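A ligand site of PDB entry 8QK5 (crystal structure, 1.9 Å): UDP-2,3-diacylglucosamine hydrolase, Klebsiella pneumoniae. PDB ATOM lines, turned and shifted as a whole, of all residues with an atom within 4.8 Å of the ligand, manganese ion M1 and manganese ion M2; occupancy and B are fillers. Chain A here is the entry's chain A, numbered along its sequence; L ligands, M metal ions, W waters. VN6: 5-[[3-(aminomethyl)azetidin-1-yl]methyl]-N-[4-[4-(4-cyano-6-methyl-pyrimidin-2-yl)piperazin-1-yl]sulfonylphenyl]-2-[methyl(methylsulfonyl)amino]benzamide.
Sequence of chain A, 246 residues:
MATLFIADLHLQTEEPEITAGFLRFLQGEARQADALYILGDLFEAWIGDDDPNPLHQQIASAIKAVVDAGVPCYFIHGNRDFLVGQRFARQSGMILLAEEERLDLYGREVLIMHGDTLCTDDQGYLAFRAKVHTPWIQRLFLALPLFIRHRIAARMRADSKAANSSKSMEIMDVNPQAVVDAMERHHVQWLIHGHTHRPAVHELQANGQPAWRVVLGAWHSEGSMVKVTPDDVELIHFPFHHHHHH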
ATOM      1  N   ASP A   8     -30.473  23.494   4.642  1.00  0.00           N
ATOM      2  CA  ASP A   8     -31.213  22.263   4.809  1.00  0.00           C
ATOM      3  C   ASP A   8     -32.640  22.452   4.320  1.00  0.00           C
ATOM      4  O   ASP A   8     -33.582  21.900   4.896  1.00  0.00           O
ATOM      5  CB  ASP A   8     -31.112  21.771   6.258  1.00  0.00           C
ATOM      6  CG  ASP A   8     -29.694  21.392   6.635  1.00  0.00           C
ATOM      7  OD1 ASP A   8     -29.144  20.466   6.000  1.00  0.00           O
ATOM      8  OD2 ASP A   8     -29.132  22.021   7.555  1.00  0.00           O
ATOM      9  N   HIS A  10     -33.421  21.235   1.290  1.00  0.00           N
ATOM     10  CA  HIS A  10     -33.689  19.974   0.596  1.00  0.00           C
ATOM     11  C   HIS A  10     -34.691  20.153  -0.553  1.00  0.00           C
ATOM     12  O   HIS A  10     -35.615  19.357  -0.723  1.00  0.00           O
ATOM     13  CB  HIS A  10     -34.119  18.898   1.604  1.00  0.00           C
ATOM     14  CG  HIS A  10     -33.035  18.603   2.585  1.00  0.00           C
ATOM     15  ND1 HIS A  10     -31.968  17.822   2.216  1.00  0.00           N
ATOM     16  CD2 HIS A  10     -32.775  19.011   3.814  1.00  0.00           C
ATOM     17  CE1 HIS A  10     -31.099  17.759   3.212  1.00  0.00           C
ATOM     18  NE2 HIS A  10     -31.554  18.492   4.192  1.00  0.00           N
ATOM     19  N   ASP A  41     -27.243  22.134   1.540  1.00  0.00           N
ATOM     20  CA  ASP A  41     -28.457  21.367   1.401  1.00  0.00           C
ATOM     21  C   ASP A  41     -29.579  22.300   0.967  1.00  0.00           C
ATOM     22  O   ASP A  41     -30.732  22.173   1.417  1.00  0.00           O
ATOM     23  CB  ASP A  41     -28.778  20.555   2.658  1.00  0.00           C
ATOM     24  CG  ASP A  41     -27.859  19.364   2.843  1.00  0.00           C
ATOM     25  OD1 ASP A  41     -26.889  19.258   2.044  1.00  0.00           O
ATOM     26  OD2 ASP A  41     -28.079  18.573   3.789  1.00  0.00           O
ATOM     27  N   GLU A  44     -32.054  18.715  -2.411  1.00  0.00           N
ATOM     28  CA  GLU A  44     -32.075  17.352  -1.904  1.00  0.00           C
ATOM     29  C   GLU A  44     -31.005  16.515  -2.582  1.00  0.00           C
ATOM     30  O   GLU A  44     -30.519  15.551  -2.006  1.00  0.00           O
ATOM     31  CB  GLU A  44     -33.462  16.742  -2.130  1.00  0.00           C
ATOM     32  CG  GLU A  44     -33.611  15.276  -1.747  1.00  0.00           C
ATOM     33  CD  GLU A  44     -33.157  14.814  -0.368  1.00  0.00           C
ATOM     34  OE1 GLU A  44     -32.821  15.655   0.498  1.00  0.00           O
ATOM     35  OE2 GLU A  44     -33.112  13.605  -0.159  1.00  0.00           O
ATOM     36  N   ALA A  45     -30.676  16.851  -3.828  1.00  0.00           N
ATOM     37  CA  ALA A  45     -29.639  16.167  -4.570  1.00  0.00           C
ATOM     38  C   ALA A  45     -29.135  17.081  -5.681  1.00  0.00           C
ATOM     39  O   ALA A  45     -29.774  18.078  -6.029  1.00  0.00           O
ATOM     40  CB  ALA A  45     -30.155  14.873  -5.131  1.00  0.00           C
ATOM     41  N   TRP A  46     -27.970  16.744  -6.209  1.00  0.00           N
ATOM     42  CA  TRP A  46     -27.386  17.491  -7.311  1.00  0.00           C
ATOM     43  C   TRP A  46     -26.398  16.584  -8.031  1.00  0.00           C
ATOM     44  O   TRP A  46     -25.504  16.039  -7.390  1.00  0.00           O
ATOM     45  CB  TRP A  46     -26.645  18.711  -6.782  1.00  0.00           C
ATOM     46  CG  TRP A  46     -26.407  19.766  -7.816  1.00  0.00           C
ATOM     47  CD1 TRP A  46     -25.306  19.921  -8.607  1.00  0.00           C
ATOM     48  CD2 TRP A  46     -27.338  20.773  -8.218  1.00  0.00           C
ATOM     49  NE1 TRP A  46     -25.471  20.983  -9.453  1.00  0.00           N
ATOM     50  CE2 TRP A  46     -26.706  21.548  -9.225  1.00  0.00           C
ATOM     51  CE3 TRP A  46     -28.638  21.115  -7.822  1.00  0.00           C
ATOM     52  CZ2 TRP A  46     -27.325  22.639  -9.818  1.00  0.00           C
ATOM     53  CZ3 TRP A  46     -29.253  22.193  -8.413  1.00  0.00           C
ATOM     54  CH2 TRP A  46     -28.600  22.948  -9.391  1.00  0.00           C
ATOM     55  N   ILE A  47     -26.595  16.432  -9.345  1.00  0.00           N
ATOM     56  CA  ILE A  47     -25.773  15.562 -10.166  1.00  0.00           C
ATOM     57  C   ILE A  47     -25.017  16.380 -11.214  1.00  0.00           C
ATOM     58  O   ILE A  47     -24.387  15.821 -12.102  1.00  0.00           O
ATOM     59  CB  ILE A  47     -26.614  14.442 -10.825  1.00  0.00           C
ATOM     60  CG1 ILE A  47     -27.701  14.998 -11.755  1.00  0.00           C
ATOM     61  CG2 ILE A  47     -27.176  13.492  -9.789  1.00  0.00           C
ATOM     62  CD1 ILE A  47     -28.418  13.911 -12.520  1.00  0.00           C
ATOM     63  N   ASN A  79     -23.844  18.160   2.228  1.00  0.00           N
ATOM     64  CA  ASN A  79     -23.495  16.795   1.882  1.00  0.00           C
ATOM     65  C   ASN A  79     -24.333  16.362   0.694  1.00  0.00           C
ATOM     66  O   ASN A  79     -23.945  15.448  -0.014  1.00  0.00           O
ATOM     67  CB  ASN A  79     -23.677  15.837   3.055  1.00  0.00           C
ATOM     68  CG  ASN A  79     -25.115  15.747   3.532  1.00  0.00           C
ATOM     69  OD1 ASN A  79     -25.608  16.722   4.055  1.00  0.00           O
ATOM     70  ND2 ASN A  79     -25.802  14.637   3.349  1.00  0.00           N
ATOM     71  N   ARG A  80     -25.481  17.025   0.491  1.00  0.00           N
ATOM     72  CA  ARG A  80     -26.410  16.634  -0.560  1.00  0.00           C
ATOM     73  C   ARG A  80     -26.032  17.299  -1.882  1.00  0.00           C
ATOM     74  O   ARG A  80     -26.263  16.693  -2.928  1.00  0.00           O
ATOM     75  CB  ARG A  80     -27.876  16.948  -0.246  1.00  0.00           C
ATOM     76  CG  ARG A  80     -28.436  16.308   1.032  1.00  0.00           C
ATOM     77  CD  ARG A  80     -28.399  14.803   1.068  1.00  0.00           C
ATOM     78  NE  ARG A  80     -29.195  14.227  -0.006  1.00  0.00           N
ATOM     79  CZ  ARG A  80     -29.349  12.927  -0.214  1.00  0.00           C
ATOM     80  NH1 ARG A  80     -28.800  12.045   0.596  1.00  0.00           N
ATOM     81  NH2 ARG A  80     -30.045  12.514  -1.259  1.00  0.00           N
ATOM     82  N   PHE A  82     -22.996  19.097  -2.831  1.00  0.00           N
ATOM     83  CA  PHE A  82     -21.594  19.389  -3.050  1.00  0.00           C
ATOM     84  C   PHE A  82     -21.209  19.578  -4.524  1.00  0.00           C
ATOM     85  O   PHE A  82     -20.164  20.139  -4.783  1.00  0.00           O
ATOM     86  CB  PHE A  82     -20.776  18.294  -2.358  1.00  0.00           C
ATOM     87  CG  PHE A  82     -21.004  16.903  -2.895  1.00  0.00           C
ATOM     88  CD1 PHE A  82     -20.312  16.454  -4.008  1.00  0.00           C
ATOM     89  CD2 PHE A  82     -21.891  16.052  -2.281  1.00  0.00           C
ATOM     90  CE1 PHE A  82     -20.512  15.177  -4.489  1.00  0.00           C
ATOM     91  CE2 PHE A  82     -22.107  14.770  -2.763  1.00  0.00           C
ATOM     92  CZ  PHE A  82     -21.416  14.342  -3.883  1.00  0.00           C
ATOM     93  N   LEU A  83     -22.063  19.192  -5.498  1.00  0.00           N
ATOM     94  CA  LEU A  83     -21.695  19.323  -6.911  1.00  0.00           C
ATOM     95  C   LEU A  83     -22.216  20.632  -7.514  1.00  0.00           C
ATOM     96  O   LEU A  83     -21.966  20.939  -8.678  1.00  0.00           O
ATOM     97  CB  LEU A  83     -22.219  18.103  -7.686  1.00  0.00           C
ATOM     98  CG  LEU A  83     -21.457  16.795  -7.447  1.00  0.00           C
ATOM     99  CD1 LEU A  83     -22.047  15.633  -8.241  1.00  0.00           C
ATOM    100  CD2 LEU A  83     -19.975  16.989  -7.803  1.00  0.00           C
ATOM    101  N   HIS A 114     -21.473  24.179   6.889  1.00  0.00           N
ATOM    102  CA  HIS A 114     -22.620  23.285   6.755  1.00  0.00           C
ATOM    103  C   HIS A 114     -22.801  22.516   8.056  1.00  0.00           C
ATOM    104  O   HIS A 114     -23.907  22.418   8.556  1.00  0.00           O
ATOM    105  CB  HIS A 114     -22.477  22.304   5.588  1.00  0.00           C
ATOM    106  CG  HIS A 114     -23.680  21.425   5.477  1.00  0.00           C
ATOM    107  ND1 HIS A 114     -24.927  21.987   5.319  1.00  0.00           N
ATOM    108  CD2 HIS A 114     -23.863  20.086   5.493  1.00  0.00           C
ATOM    109  CE1 HIS A 114     -25.818  21.001   5.212  1.00  0.00           C
ATOM    110  NE2 HIS A 114     -25.205  19.834   5.311  1.00  0.00           N
ATOM    111  N   ASP A 122     -19.113   9.702  12.545  1.00  0.00           N
ATOM    112  CA  ASP A 122     -19.633   8.914  11.454  1.00  0.00           C
ATOM    113  C   ASP A 122     -18.504   8.696  10.448  1.00  0.00           C
ATOM    114  O   ASP A 122     -18.299   9.528   9.566  1.00  0.00           O
ATOM    115  CB  ASP A 122     -20.847   9.597  10.839  1.00  0.00           C
ATOM    116  CG  ASP A 122     -21.682   8.702   9.937  1.00  0.00           C
ATOM    117  OD1 ASP A 122     -21.205   7.590   9.602  1.00  0.00           O
ATOM    118  OD2 ASP A 122     -22.802   9.114   9.587  1.00  0.00           O
ATOM    119  N   GLY A 124     -18.394   6.174   8.379  1.00  0.00           N
ATOM    120  CA  GLY A 124     -19.223   5.935   7.221  1.00  0.00           C
ATOM    121  C   GLY A 124     -19.241   7.174   6.330  1.00  0.00           C
ATOM    122  O   GLY A 124     -18.669   7.177   5.247  1.00  0.00           O
ATOM    123  N   TYR A 125     -19.821   8.241   6.857  1.00  0.00           N
ATOM    124  CA  TYR A 125     -20.075   9.433   6.087  1.00  0.00           C
ATOM    125  C   TYR A 125     -18.754  10.094   5.683  1.00  0.00           C
ATOM    126  O   TYR A 125     -18.657  10.630   4.585  1.00  0.00           O
ATOM    127  CB  TYR A 125     -20.962  10.430   6.834  1.00  0.00           C
ATOM    128  CG  TYR A 125     -21.004  11.743   6.107  1.00  0.00           C
ATOM    129  CD1 TYR A 125     -21.628  11.846   4.872  1.00  0.00           C
ATOM    130  CD2 TYR A 125     -20.304  12.835   6.566  1.00  0.00           C
ATOM    131  CE1 TYR A 125     -21.615  13.018   4.136  1.00  0.00           C
ATOM    132  CE2 TYR A 125     -20.267  14.017   5.850  1.00  0.00           C
ATOM    133  CZ  TYR A 125     -20.923  14.104   4.625  1.00  0.00           C
ATOM    134  OH  TYR A 125     -20.869  15.260   3.896  1.00  0.00           O
ATOM    135  N   PHE A 128     -16.978   8.465   2.703  1.00  0.00           N
ATOM    136  CA  PHE A 128     -17.779   8.881   1.557  1.00  0.00           C
ATOM    137  C   PHE A 128     -17.438  10.306   1.126  1.00  0.00           C
ATOM    138  O   PHE A 128     -17.217  10.578  -0.059  1.00  0.00           O
ATOM    139  CB  PHE A 128     -19.265   8.690   1.892  1.00  0.00           C
ATOM    140  CG  PHE A 128     -20.244   9.330   0.941  1.00  0.00           C
ATOM    141  CD1 PHE A 128     -20.816   8.607  -0.097  1.00  0.00           C
ATOM    142  CD2 PHE A 128     -20.626  10.653   1.109  1.00  0.00           C
ATOM    143  CE1 PHE A 128     -21.721   9.201  -0.955  1.00  0.00           C
ATOM    144  CE2 PHE A 128     -21.516  11.258   0.239  1.00  0.00           C
ATOM    145  CZ  PHE A 128     -22.076  10.532  -0.792  1.00  0.00           C
ATOM    146  N   VAL A 132     -16.089  11.779  -2.504  1.00  0.00           N
ATOM    147  CA  VAL A 132     -16.893  12.589  -3.396  1.00  0.00           C
ATOM    148  C   VAL A 132     -16.393  14.024  -3.413  1.00  0.00           C
ATOM    149  O   VAL A 132     -16.823  14.820  -4.256  1.00  0.00           O
ATOM    150  CB  VAL A 132     -18.406  12.504  -3.091  1.00  0.00           C
ATOM    151  CG1 VAL A 132     -18.909  11.087  -3.159  1.00  0.00           C
ATOM    152  CG2 VAL A 132     -18.783  13.125  -1.747  1.00  0.00           C
ATOM    153  N   ILE A 137     -12.572  12.638  -8.859  1.00  0.00           N
ATOM    154  CA  ILE A 137     -13.741  11.780  -8.785  1.00  0.00           C
ATOM    155  C   ILE A 137     -14.982  12.592  -9.159  1.00  0.00           C
ATOM    156  O   ILE A 137     -15.899  12.056  -9.757  1.00  0.00           O
ATOM    157  CB  ILE A 137     -13.848  11.097  -7.419  1.00  0.00           C
ATOM    158  CG1 ILE A 137     -12.770  10.011  -7.287  1.00  0.00           C
ATOM    159  CG2 ILE A 137     -15.242  10.556  -7.176  1.00  0.00           C
ATOM    160  CD1 ILE A 137     -12.787   9.261  -5.969  1.00  0.00           C
ATOM    161  N   GLN A 138     -14.974  13.900  -8.881  1.00  0.00           N
ATOM    162  CA  GLN A 138     -16.054  14.774  -9.296  1.00  0.00           C
ATOM    163  C   GLN A 138     -16.050  14.945 -10.817  1.00  0.00           C
ATOM    164  O   GLN A 138     -17.108  14.842 -11.415  1.00  0.00           O
ATOM    165  CB  GLN A 138     -15.974  16.106  -8.564  1.00  0.00           C
ATOM    166  CG  GLN A 138     -16.273  15.968  -7.079  1.00  0.00           C
ATOM    167  CD  GLN A 138     -16.443  17.283  -6.368  1.00  0.00           C
ATOM    168  OE1 GLN A 138     -16.195  18.354  -6.925  1.00  0.00           O
ATOM    169  NE2 GLN A 138     -16.923  17.212  -5.125  1.00  0.00           N
ATOM    170  N   PHE A 141     -17.379  11.874 -12.538  1.00  0.00           N
ATOM    171  CA  PHE A 141     -18.810  11.642 -12.415  1.00  0.00           C
ATOM    172  C   PHE A 141     -19.543  12.572 -13.366  1.00  0.00           C
ATOM    173  O   PHE A 141     -20.488  12.154 -14.019  1.00  0.00           O
ATOM    174  CB  PHE A 141     -19.321  11.877 -10.993  1.00  0.00           C
ATOM    175  CG  PHE A 141     -20.800  11.744 -10.794  1.00  0.00           C
ATOM    176  CD1 PHE A 141     -21.396  10.502 -10.614  1.00  0.00           C
ATOM    177  CD2 PHE A 141     -21.612  12.873 -10.748  1.00  0.00           C
ATOM    178  CE1 PHE A 141     -22.760  10.387 -10.397  1.00  0.00           C
ATOM    179  CE2 PHE A 141     -22.972  12.760 -10.522  1.00  0.00           C
ATOM    180  CZ  PHE A 141     -23.544  11.519 -10.342  1.00  0.00           C
ATOM    181  N   ILE A 152     -27.197   6.352 -11.369  1.00  0.00           N
ATOM    182  CA  ILE A 152     -26.282   6.202 -10.243  1.00  0.00           C
ATOM    183  C   ILE A 152     -26.901   6.759  -8.955  1.00  0.00           C
ATOM    184  O   ILE A 152     -26.908   6.086  -7.919  1.00  0.00           O
ATOM    185  CB  ILE A 152     -24.922   6.854 -10.582  1.00  0.00           C
ATOM    186  CG1 ILE A 152     -24.091   5.951 -11.503  1.00  0.00           C
ATOM    187  CG2 ILE A 152     -24.149   7.223  -9.320  1.00  0.00           C
ATOM    188  CD1 ILE A 152     -22.769   6.538 -11.954  1.00  0.00           C
ATOM    189  N   ALA A 153     -27.437   7.982  -9.040  1.00  0.00           N
ATOM    190  CA  ALA A 153     -28.029   8.671  -7.897  1.00  0.00           C
ATOM    191  C   ALA A 153     -29.213   7.880  -7.338  1.00  0.00           C
ATOM    192  O   ALA A 153     -29.408   7.867  -6.127  1.00  0.00           O
ATOM    193  CB  ALA A 153     -28.413  10.068  -8.282  1.00  0.00           C
ATOM    194  N   MET A 156     -28.851   5.859  -4.409  1.00  0.00           N
ATOM    195  CA  MET A 156     -28.380   6.678  -3.303  1.00  0.00           C
ATOM    196  C   MET A 156     -29.555   7.470  -2.710  1.00  0.00           C
ATOM    197  O   MET A 156     -30.213   6.903  -1.821  1.00  0.00           O
ATOM    198  CB  MET A 156     -27.295   7.642  -3.784  1.00  0.00           C
ATOM    199  CG  MET A 156     -26.202   6.944  -4.595  1.00  0.00           C
ATOM    200  SD  MET A 156     -24.556   7.628  -4.277  1.00  0.00           S
ATOM    201  CE  MET A 156     -23.806   7.638  -5.903  1.00  0.00           C
ATOM    202  N   ILE A 171     -29.439  11.498  10.938  1.00  0.00           N
ATOM    203  CA  ILE A 171     -28.192  12.180  10.646  1.00  0.00           C
ATOM    204  C   ILE A 171     -27.373  12.255  11.949  1.00  0.00           C
ATOM    205  O   ILE A 171     -27.867  12.727  12.980  1.00  0.00           O
ATOM    206  CB  ILE A 171     -28.483  13.539   9.971  1.00  0.00           C
ATOM    207  CG1 ILE A 171     -29.259  13.320   8.665  1.00  0.00           C
ATOM    208  CG2 ILE A 171     -27.215  14.350   9.757  1.00  0.00           C
ATOM    209  CD1 ILE A 171     -29.475  14.547   7.830  1.00  0.00           C
ATOM    210  N   HIS A 195     -26.932  20.999   8.728  1.00  0.00           N
ATOM    211  CA  HIS A 195     -26.610  19.593   8.534  1.00  0.00           C
ATOM    212  C   HIS A 195     -27.384  18.649   9.466  1.00  0.00           C
ATOM    213  O   HIS A 195     -27.946  17.661   8.999  1.00  0.00           O
ATOM    214  CB  HIS A 195     -25.119  19.316   8.659  1.00  0.00           C
ATOM    215  CG  HIS A 195     -24.874  17.880   8.317  1.00  0.00           C
ATOM    216  ND1 HIS A 195     -25.254  17.309   7.114  1.00  0.00           N
ATOM    217  CD2 HIS A 195     -24.415  16.890   9.098  1.00  0.00           C
ATOM    218  CE1 HIS A 195     -24.894  16.028   7.142  1.00  0.00           C
ATOM    219  NE2 HIS A 195     -24.420  15.745   8.343  1.00  0.00           N
ATOM    220  N   HIS A 197     -30.114  19.009  11.332  1.00  0.00           N
ATOM    221  CA  HIS A 197     -31.572  19.133  11.386  1.00  0.00           C
ATOM    222  C   HIS A 197     -32.091  19.114  12.830  1.00  0.00           C
ATOM    223  O   HIS A 197     -33.226  18.700  13.056  1.00  0.00           O
ATOM    224  CB  HIS A 197     -32.254  18.024  10.587  1.00  0.00           C
ATOM    225  CG  HIS A 197     -31.797  17.914   9.167  1.00  0.00           C
ATOM    226  ND1 HIS A 197     -32.195  16.879   8.343  1.00  0.00           N
ATOM    227  CD2 HIS A 197     -30.974  18.683   8.435  1.00  0.00           C
ATOM    228  CE1 HIS A 197     -31.604  17.017   7.164  1.00  0.00           C
ATOM    229  NE2 HIS A 197     -30.868  18.108   7.190  1.00  0.00           N
HETATM  230  C5  VN6 L   1     -19.702  11.692  -7.268  1.00  0.00           C
HETATM  231  C6  VN6 L   1     -19.490  10.361  -7.533  1.00  0.00           C
HETATM  232  N7  VN6 L   1     -23.214  11.625  -6.457  1.00  0.00           N
HETATM  233  C8  VN6 L   1     -23.463  13.064  -6.529  1.00  0.00           C
HETATM  234  C26 VN6 L   1     -23.776   9.240   2.798  1.00  0.00           C
HETATM  235  C27 VN6 L   1     -23.484   8.410   3.893  1.00  0.00           C
HETATM  236  C28 VN6 L   1     -24.014   8.699   5.146  1.00  0.00           C
HETATM  237  C29 VN6 L   1     -24.834   9.806   5.330  1.00  0.00           C
HETATM  238  C30 VN6 L   1     -25.157  10.629   4.264  1.00  0.00           C
HETATM  239  C32 VN6 L   1     -25.855  12.258   5.908  1.00  0.00           C
HETATM  240  C37 VN6 L   1     -18.560  12.715  -7.332  1.00  0.00           C
HETATM  241  C38 VN6 L   1     -20.354   8.087  -7.687  1.00  0.00           C
HETATM  242  C40 VN6 L   1     -22.575   7.230   3.790  1.00  0.00           C
HETATM  243  C42 VN6 L   1     -22.002   5.125   2.916  1.00  0.00           C
HETATM  244  C1  VN6 L   1     -20.539   9.470  -7.439  1.00  0.00           C
HETATM  245  N2  VN6 L   1     -21.753   9.905  -7.114  1.00  0.00           N
HETATM  246  C3  VN6 L   1     -21.976  11.222  -6.931  1.00  0.00           C
HETATM  247  N4  VN6 L   1     -20.945  12.103  -6.944  1.00  0.00           N
HETATM  248  C9  VN6 L   1     -24.513  13.353  -5.456  1.00  0.00           C
HETATM  249  C10 VN6 L   1     -24.315  10.866  -6.920  1.00  0.00           C
HETATM  250  C11 VN6 L   1     -25.455  11.076  -5.894  1.00  0.00           C
HETATM  251  N12 VN6 L   1     -25.743  12.560  -5.752  1.00  0.00           N
HETATM  252  S13 VN6 L   1     -26.947  12.858  -4.639  1.00  0.00           S
HETATM  253  C14 VN6 L   1     -26.481  12.262  -3.064  1.00  0.00           C
HETATM  254  O15 VN6 L   1     -27.180  14.271  -4.607  1.00  0.00           O
HETATM  255  O16 VN6 L   1     -28.110  12.165  -5.079  1.00  0.00           O
HETATM  256  C17 VN6 L   1     -26.827  10.989  -2.722  1.00  0.00           C
HETATM  257  C18 VN6 L   1     -26.476  10.481  -1.498  1.00  0.00           C
HETATM  258  C19 VN6 L   1     -25.752  11.230  -0.578  1.00  0.00           C
HETATM  259  C20 VN6 L   1     -25.718  13.060  -2.156  1.00  0.00           C
HETATM  260  C21 VN6 L   1     -25.349  12.510  -0.904  1.00  0.00           C
HETATM  261  N22 VN6 L   1     -25.363  10.603   0.617  1.00  0.00           N
HETATM  262  C23 VN6 L   1     -24.945  11.245   1.756  1.00  0.00           C
HETATM  263  O24 VN6 L   1     -24.861  12.478   1.798  1.00  0.00           O
HETATM  264  C25 VN6 L   1     -24.584  10.366   2.981  1.00  0.00           C
HETATM  265  N31 VN6 L   1     -25.969  11.811   4.480  1.00  0.00           N
HETATM  266  S33 VN6 L   1     -27.533  11.536   4.104  1.00  0.00           S
HETATM  267  C34 VN6 L   1     -28.240  10.375   5.263  1.00  0.00           C
HETATM  268  O35 VN6 L   1     -28.217  12.789   4.153  1.00  0.00           O
HETATM  269  O36 VN6 L   1     -27.631  11.009   2.771  1.00  0.00           O
HETATM  270  N39 VN6 L   1     -20.229   6.986  -7.873  1.00  0.00           N
HETATM  271  N41 VN6 L   1     -22.967   6.271   2.791  1.00  0.00           N
HETATM  272  C43 VN6 L   1     -24.078   5.413   3.287  1.00  0.00           C
HETATM  273  C44 VN6 L   1     -23.205   4.193   3.029  1.00  0.00           C
HETATM  274  C45 VN6 L   1     -23.513   3.636   1.637  1.00  0.00           C
HETATM  275  N46 VN6 L   1     -23.393   2.167   1.632  1.00  0.00           N
HETATM  276 MN    MN M   1     -26.625  18.039   5.384  1.00  0.00          MN
HETATM  277 MN    MN M   2     -29.643  18.485   5.358  1.00  0.00          MN
HETATM  278  O   HOH W   1     -28.374  17.109   6.382  1.00  0.00           O
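Within 4 Å of manganese ion M2: Asp 8, His 10, Asp 41 and His 197. The nearest printed residue that does not touch manganese ion M2 is His 195 (4.1 Å).
Manganese ion M1 is bound by the side-chain amide oxygen (OD1) of Asn 79 (2.1 Å), water W1 (2.2 Å), the side-chain carboxylate (OD2) of Asp 41 (2.2 Å), a ring nitrogen (NE2) of His 114 (2.3 Å) and a ring nitrogen (ND1) of His 195 (2.3 Å).
The nearest printed residue that does not touch manganese ion M1 is His 197 (4.6 Å).
An oxygen (O24) of the ligand is in hydrogen-bond range of the side-chain amide nitrogen (ND2) of Asn 79, 2.8 Å away. The guanidinium group of Arg 80 sits at hydrogen-bond distance from an oxygen (O36) of the ligand (2.7 Å). The backbone NH of Trp 46 sits at hydrogen-bond distance from an oxygen (O15) of the ligand (3.1 Å).
The guanidinium group (NH2) of Arg 80 lies within salt-bridge range of the side-chain carboxylate (OE2) of Glu 44 (3.4 Å). NE2 of Gln 138 is in hydrogen-bond range of O of Val 132 (2.5 Å). A ring nitrogen (NE2) of His 197 sits close to the backbone carbonyl oxygen (O) of His 195, 3.5 Å away. A ring nitrogen (ND1) of His 10 is in hydrogen-bond range of the side-chain carboxylate (OE1) of Glu 44 (2.9 Å). N of His 195 lies within hydrogen-bond range of OD2 of Asp 8 (2.7 Å). The backbone NH (N) of Arg 80 lies within hydrogen-bond range of the side-chain carboxylate (OD1) of Asp 41, 3.1 Å away. N of Tyr 125 sits at hydrogen-bond distance from OD1 of Asp 122 (3.1 Å).
Manganese ion M2 is bound by water W1 (2.1 Å), the side-chain carboxylate of Asp 8 (2.1 Å), the side-chain carboxylate of Asp 41 (2.2 Å), a ring nitrogen (NE2) of His 197 (2.2 Å) and a ring nitrogen (NE2) of His 10 (2.2 Å).
Ala 45 touches the ligand. Phe 82 touches the ligand. CD1 of Leu 83 touches C8 of the ligand, 3.4 Å away. Tyr 125 touches the ligand. Phe 128 touches the ligand. O of Ile 137 touches C37 of the ligand (3.7 Å). CA of Gln 138 touches C37 of the ligand, at 3.8 Å. Phe 141 touches the ligand (CD1 to C1, 3.4 Å). Ala 153 touches the ligand (CB to O16, 3.8 Å). Met 156 touches the ligand (CE to N2, 3.3 Å). Hydrophobic or aromatic side chains within 4 Å of the ligand: Ala 45, Phe 82, Leu 83, Tyr 125, Phe 128, Ile 137, Phe 141, Ala 153 and Met 156.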
